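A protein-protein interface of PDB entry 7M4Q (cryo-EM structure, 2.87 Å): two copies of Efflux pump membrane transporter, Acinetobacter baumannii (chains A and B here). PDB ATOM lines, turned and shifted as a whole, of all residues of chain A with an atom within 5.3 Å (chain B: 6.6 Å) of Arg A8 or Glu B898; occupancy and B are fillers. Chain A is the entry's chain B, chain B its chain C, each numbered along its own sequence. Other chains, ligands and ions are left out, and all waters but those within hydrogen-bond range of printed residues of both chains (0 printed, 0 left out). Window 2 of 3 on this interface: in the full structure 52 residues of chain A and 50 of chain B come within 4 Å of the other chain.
The side-chain carboxylate (OE2) of Glu B898 is in hydrogen-bond range of the backbone NH (N) of Ile A10 (3.4 Å). OE2 of Glu B898 lies within hydrogen-bond range of N of Phe A11 (3.2 Å). OE2 of Glu B898 lies close to O of Arg A8.
NH2 of Arg A8 is in hydrogen-bond range of O of Phe A4 (3.0 Å). The backbone carbonyl oxygen (O) of Tyr B897 sits at hydrogen-bond distance from the side-chain hydroxyl (OG) of Ser B899, 3.4 Å away.
Among the printed residues, merely in contact across the chains: Pro A9 with Glu B898 (3.6 Å), Ile A10 with Trp B900 (3.7 Å), Phe A11 with Ala B895 (3.8 Å) and Ile A10 with Ser B899 (3.9 Å).
Of chain B, only Glu B898 (2.9 Å) comes within 4 Å of Arg A8. Glu B898 touches just these residues of chain A: Arg A8, Pro A9, Ile A10 and Phe A11. Of the printed residues of chain B, Ile A10 touches Glu B898, Ser B899 and Trp B900. Printed residues of chain A within 4 Å of Trp B900: Ile A10. Printed residues of chain A within 4 Å of Ser B899: Ile A10. Ala A491 touches none of the printed residues of chain B. Phe A4 touches none of the printed residues of chain B. The nearest residue of chain A that does not touch Glu B898 is His A7 (4.6 Å).
Printed residues of chain B that touch a printed residue of chain A: Ala B895, Glu B898, Ser B899 and Trp B900. Printed residues of chain A that touch a printed residue of chain B: Arg A8, Pro A9, Ile A10 and Phe A11. Hydrophobic or aromatic side chains of chain A within 4 Å of the printed part of chain B: Pro A9, Ile A10 and Phe A11.
No position is printed for both chains. Of the 7 pairs that touch across the chains among the printed residues, none has its exchanged pair printed and touching as well.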
ATOM      1  N   PHE A   4     -37.162   8.368   5.087  1.00  0.00           N
ATOM      2  CA  PHE A   4     -35.711   8.241   5.043  1.00  0.00           C
ATOM      3  C   PHE A   4     -35.152   8.581   3.665  1.00  0.00           C
ATOM      4  O   PHE A   4     -34.096   9.207   3.559  1.00  0.00           O
ATOM      5  CB  PHE A   4     -35.318   6.827   5.461  1.00  0.00           C
ATOM      6  CG  PHE A   4     -33.869   6.533   5.301  1.00  0.00           C
ATOM      7  CD1 PHE A   4     -32.967   6.906   6.267  1.00  0.00           C
ATOM      8  CD2 PHE A   4     -33.402   5.883   4.180  1.00  0.00           C
ATOM      9  CE1 PHE A   4     -31.641   6.643   6.118  1.00  0.00           C
ATOM     10  CE2 PHE A   4     -32.069   5.617   4.034  1.00  0.00           C
ATOM     11  CZ  PHE A   4     -31.192   5.997   5.006  1.00  0.00           C
ATOM     12  N   PHE A   5     -35.848   8.193   2.598  1.00  0.00           N
ATOM     13  CA  PHE A   5     -35.342   8.396   1.250  1.00  0.00           C
ATOM     14  C   PHE A   5     -35.754   9.723   0.637  1.00  0.00           C
ATOM     15  O   PHE A   5     -35.197  10.108  -0.395  1.00  0.00           O
ATOM     16  CB  PHE A   5     -35.786   7.247   0.349  1.00  0.00           C
ATOM     17  CG  PHE A   5     -35.091   5.964   0.649  1.00  0.00           C
ATOM     18  CD1 PHE A   5     -33.826   5.723   0.162  1.00  0.00           C
ATOM     19  CD2 PHE A   5     -35.683   5.014   1.445  1.00  0.00           C
ATOM     20  CE1 PHE A   5     -33.176   4.551   0.451  1.00  0.00           C
ATOM     21  CE2 PHE A   5     -35.035   3.845   1.736  1.00  0.00           C
ATOM     22  CZ  PHE A   5     -33.782   3.616   1.239  1.00  0.00           C
ATOM     23  N   ILE A   6     -36.697  10.441   1.240  1.00  0.00           N
ATOM     24  CA  ILE A   6     -36.981  11.797   0.788  1.00  0.00           C
ATOM     25  C   ILE A   6     -35.741  12.666   0.934  1.00  0.00           C
ATOM     26  O   ILE A   6     -35.506  13.582   0.140  1.00  0.00           O
ATOM     27  CB  ILE A   6     -38.169  12.377   1.569  1.00  0.00           C
ATOM     28  CG1 ILE A   6     -39.447  11.649   1.188  1.00  0.00           C
ATOM     29  CG2 ILE A   6     -38.313  13.863   1.301  1.00  0.00           C
ATOM     30  CD1 ILE A   6     -40.616  11.989   2.067  1.00  0.00           C
ATOM     31  N   HIS A   7     -34.940  12.407   1.958  1.00  0.00           N
ATOM     32  CA  HIS A   7     -33.754  13.191   2.249  1.00  0.00           C
ATOM     33  C   HIS A   7     -32.477  12.519   1.783  1.00  0.00           C
ATOM     34  O   HIS A   7     -31.391  12.972   2.137  1.00  0.00           O
ATOM     35  CB  HIS A   7     -33.695  13.476   3.744  1.00  0.00           C
ATOM     36  CG  HIS A   7     -34.866  14.261   4.244  1.00  0.00           C
ATOM     37  ND1 HIS A   7     -35.520  13.959   5.414  1.00  0.00           N
ATOM     38  CD2 HIS A   7     -35.504  15.332   3.721  1.00  0.00           C
ATOM     39  CE1 HIS A   7     -36.504  14.819   5.599  1.00  0.00           C
ATOM     40  NE2 HIS A   7     -36.517  15.661   4.583  1.00  0.00           N
ATOM     41  N   ARG A   8     -32.582  11.445   1.006  1.00  0.00           N
ATOM     42  CA  ARG A   8     -31.426  10.720   0.482  1.00  0.00           C
ATOM     43  C   ARG A   8     -31.740  10.210  -0.917  1.00  0.00           C
ATOM     44  O   ARG A   8     -31.809   9.003  -1.157  1.00  0.00           O
ATOM     45  CB  ARG A   8     -31.062   9.571   1.416  1.00  0.00           C
ATOM     46  CG  ARG A   8     -30.539  10.026   2.734  1.00  0.00           C
ATOM     47  CD  ARG A   8     -30.199   8.857   3.598  1.00  0.00           C
ATOM     48  NE  ARG A   8     -29.794   9.289   4.927  1.00  0.00           N
ATOM     49  CZ  ARG A   8     -30.634   9.748   5.847  1.00  0.00           C
ATOM     50  NH1 ARG A   8     -30.175  10.121   7.033  1.00  0.00           N
ATOM     51  NH2 ARG A   8     -31.932   9.840   5.584  1.00  0.00           N
ATOM     52  N   PRO A   9     -31.938  11.114  -1.874  1.00  0.00           N
ATOM     53  CA  PRO A   9     -32.302  10.669  -3.228  1.00  0.00           C
ATOM     54  C   PRO A   9     -31.263   9.782  -3.895  1.00  0.00           C
ATOM     55  O   PRO A   9     -31.610   8.896  -4.680  1.00  0.00           O
ATOM     56  CB  PRO A   9     -32.478  11.993  -3.982  1.00  0.00           C
ATOM     57  CG  PRO A   9     -32.624  13.011  -2.964  1.00  0.00           C
ATOM     58  CD  PRO A   9     -31.875  12.575  -1.780  1.00  0.00           C
ATOM     59  N   ILE A  10     -29.983  10.021  -3.629  1.00  0.00           N
ATOM     60  CA  ILE A  10     -28.943   9.279  -4.321  1.00  0.00           C
ATOM     61  C   ILE A  10     -28.878   7.839  -3.831  1.00  0.00           C
ATOM     62  O   ILE A  10     -28.573   6.927  -4.605  1.00  0.00           O
ATOM     63  CB  ILE A  10     -27.613  10.027  -4.160  1.00  0.00           C
ATOM     64  CG1 ILE A  10     -27.802  11.465  -4.649  1.00  0.00           C
ATOM     65  CG2 ILE A  10     -26.507   9.328  -4.928  1.00  0.00           C
ATOM     66  CD1 ILE A  10     -26.540  12.157  -5.066  1.00  0.00           C
ATOM     67  N   PHE A  11     -29.150   7.608  -2.553  1.00  0.00           N
ATOM     68  CA  PHE A  11     -29.252   6.246  -2.049  1.00  0.00           C
ATOM     69  C   PHE A  11     -30.323   5.471  -2.810  1.00  0.00           C
ATOM     70  O   PHE A  11     -30.116   4.318  -3.211  1.00  0.00           O
ATOM     71  CB  PHE A  11     -29.564   6.309  -0.554  1.00  0.00           C
ATOM     72  CG  PHE A  11     -29.061   5.145   0.238  1.00  0.00           C
ATOM     73  CD1 PHE A  11     -29.083   3.868  -0.271  1.00  0.00           C
ATOM     74  CD2 PHE A  11     -28.578   5.338   1.504  1.00  0.00           C
ATOM     75  CE1 PHE A  11     -28.641   2.821   0.463  1.00  0.00           C
ATOM     76  CE2 PHE A  11     -28.123   4.289   2.238  1.00  0.00           C
ATOM     77  CZ  PHE A  11     -28.158   3.029   1.718  1.00  0.00           C
ATOM     78  N   ALA A  12     -31.480   6.102  -3.030  1.00  0.00           N
ATOM     79  CA  ALA A  12     -32.557   5.448  -3.761  1.00  0.00           C
ATOM     80  C   ALA A  12     -32.181   5.219  -5.216  1.00  0.00           C
ATOM     81  O   ALA A  12     -32.505   4.174  -5.788  1.00  0.00           O
ATOM     82  CB  ALA A  12     -33.831   6.275  -3.662  1.00  0.00           C
ATOM     83  N   ALA A 491     -38.689   9.538  -3.530  1.00  0.00           N
ATOM     84  CA  ALA A 491     -37.508  10.354  -3.796  1.00  0.00           C
ATOM     85  C   ALA A 491     -37.593  11.038  -5.153  1.00  0.00           C
ATOM     86  O   ALA A 491     -37.200  12.198  -5.286  1.00  0.00           O
ATOM     87  CB  ALA A 491     -36.252   9.496  -3.702  1.00  0.00           C
ATOM     88  N   LEU B 893     -19.799   4.243  -2.151  1.00  0.00           N
ATOM     89  CA  LEU B 893     -19.394   5.594  -1.797  1.00  0.00           C
ATOM     90  C   LEU B 893     -20.502   6.584  -2.098  1.00  0.00           C
ATOM     91  O   LEU B 893     -20.756   7.501  -1.312  1.00  0.00           O
ATOM     92  CB  LEU B 893     -18.127   5.987  -2.550  1.00  0.00           C
ATOM     93  CG  LEU B 893     -16.807   5.428  -2.049  1.00  0.00           C
ATOM     94  CD1 LEU B 893     -15.697   5.988  -2.895  1.00  0.00           C
ATOM     95  CD2 LEU B 893     -16.591   5.747  -0.585  1.00  0.00           C
ATOM     96  N   ALA B 894     -21.166   6.426  -3.240  1.00  0.00           N
ATOM     97  CA  ALA B 894     -22.258   7.330  -3.565  1.00  0.00           C
ATOM     98  C   ALA B 894     -23.363   7.237  -2.525  1.00  0.00           C
ATOM     99  O   ALA B 894     -23.858   8.259  -2.039  1.00  0.00           O
ATOM    100  CB  ALA B 894     -22.795   7.021  -4.958  1.00  0.00           C
ATOM    101  N   ALA B 895     -23.748   6.020  -2.152  1.00  0.00           N
ATOM    102  CA  ALA B 895     -24.840   5.862  -1.198  1.00  0.00           C
ATOM    103  C   ALA B 895     -24.481   6.436   0.166  1.00  0.00           C
ATOM    104  O   ALA B 895     -25.300   7.118   0.789  1.00  0.00           O
ATOM    105  CB  ALA B 895     -25.217   4.390  -1.072  1.00  0.00           C
ATOM    106  N   LEU B 896     -23.267   6.172   0.648  1.00  0.00           N
ATOM    107  CA  LEU B 896     -22.915   6.554   2.013  1.00  0.00           C
ATOM    108  C   LEU B 896     -22.784   8.061   2.173  1.00  0.00           C
ATOM    109  O   LEU B 896     -23.170   8.610   3.208  1.00  0.00           O
ATOM    110  CB  LEU B 896     -21.610   5.878   2.432  1.00  0.00           C
ATOM    111  CG  LEU B 896     -21.668   4.403   2.825  1.00  0.00           C
ATOM    112  CD1 LEU B 896     -20.388   4.031   3.518  1.00  0.00           C
ATOM    113  CD2 LEU B 896     -22.859   4.105   3.722  1.00  0.00           C
ATOM    114  N   TYR B 897     -22.230   8.748   1.182  1.00  0.00           N
ATOM    115  CA  TYR B 897     -21.941  10.165   1.314  1.00  0.00           C
ATOM    116  C   TYR B 897     -22.893  11.041   0.523  1.00  0.00           C
ATOM    117  O   TYR B 897     -22.672  12.251   0.436  1.00  0.00           O
ATOM    118  CB  TYR B 897     -20.497  10.445   0.907  1.00  0.00           C
ATOM    119  CG  TYR B 897     -19.532   9.779   1.839  1.00  0.00           C
ATOM    120  CD1 TYR B 897     -19.201  10.360   3.042  1.00  0.00           C
ATOM    121  CD2 TYR B 897     -18.988   8.549   1.540  1.00  0.00           C
ATOM    122  CE1 TYR B 897     -18.347   9.757   3.902  1.00  0.00           C
ATOM    123  CE2 TYR B 897     -18.131   7.934   2.406  1.00  0.00           C
ATOM    124  CZ  TYR B 897     -17.818   8.543   3.585  1.00  0.00           C
ATOM    125  OH  TYR B 897     -16.956   7.940   4.461  1.00  0.00           O
ATOM    126  N   GLU B 898     -23.955  10.473  -0.034  1.00  0.00           N
ATOM    127  CA  GLU B 898     -25.012  11.258  -0.656  1.00  0.00           C
ATOM    128  C   GLU B 898     -24.445  12.263  -1.651  1.00  0.00           C
ATOM    129  O   GLU B 898     -24.783  13.444  -1.649  1.00  0.00           O
ATOM    130  CB  GLU B 898     -25.852  11.956   0.410  1.00  0.00           C
ATOM    131  CG  GLU B 898     -27.101  11.196   0.782  1.00  0.00           C
ATOM    132  CD  GLU B 898     -28.057  11.075  -0.379  1.00  0.00           C
ATOM    133  OE1 GLU B 898     -28.094  11.997  -1.216  1.00  0.00           O
ATOM    134  OE2 GLU B 898     -28.752  10.049  -0.465  1.00  0.00           O
ATOM    135  N   SER B 899     -23.578  11.767  -2.526  1.00  0.00           N
ATOM    136  CA  SER B 899     -22.894  12.603  -3.495  1.00  0.00           C
ATOM    137  C   SER B 899     -22.609  11.787  -4.743  1.00  0.00           C
ATOM    138  O   SER B 899     -22.756  10.566  -4.759  1.00  0.00           O
ATOM    139  CB  SER B 899     -21.584  13.162  -2.933  1.00  0.00           C
ATOM    140  OG  SER B 899     -21.808  14.315  -2.147  1.00  0.00           O
ATOM    141  N   TRP B 900     -22.235  12.488  -5.804  1.00  0.00           N
ATOM    142  CA  TRP B 900     -21.575  11.866  -6.940  1.00  0.00           C
ATOM    143  C   TRP B 900     -20.134  12.316  -7.096  1.00  0.00           C
ATOM    144  O   TRP B 900     -19.335  11.596  -7.684  1.00  0.00           O
ATOM    145  CB  TRP B 900     -22.331  12.165  -8.241  1.00  0.00           C
ATOM    146  CG  TRP B 900     -23.689  11.535  -8.352  1.00  0.00           C
ATOM    147  CD1 TRP B 900     -24.871  12.181  -8.489  1.00  0.00           C
ATOM    148  CD2 TRP B 900     -23.998  10.137  -8.355  1.00  0.00           C
ATOM    149  NE1 TRP B 900     -25.896  11.284  -8.574  1.00  0.00           N
ATOM    150  CE2 TRP B 900     -25.385  10.021  -8.496  1.00  0.00           C
ATOM    151  CE3 TRP B 900     -23.234   8.973  -8.255  1.00  0.00           C
ATOM    152  CZ2 TRP B 900     -26.027   8.793  -8.534  1.00  0.00           C
ATOM    153  CZ3 TRP B 900     -23.880   7.756  -8.291  1.00  0.00           C
ATOM    154  CH2 TRP B 900     -25.256   7.675  -8.426  1.00  0.00           C
ATOM    155  N   LYS B 962     -15.307  17.196   3.577  1.00  0.00           N
ATOM    156  CA  LYS B 962     -16.705  17.481   3.287  1.00  0.00           C
ATOM    157  C   LYS B 962     -17.423  17.972   4.526  1.00  0.00           C
ATOM    158  O   LYS B 962     -18.200  18.928   4.459  1.00  0.00           O
ATOM    159  CB  LYS B 962     -17.391  16.238   2.722  1.00  0.00           C
ATOM    160  CG  LYS B 962     -18.890  16.216   2.935  1.00  0.00           C
ATOM    161  CD  LYS B 962     -19.578  15.241   2.018  1.00  0.00           C
ATOM    162  CE  LYS B 962     -21.085  15.326   2.153  1.00  0.00           C
ATOM    163  NZ  LYS B 962     -21.551  14.939   3.507  1.00  0.00           N
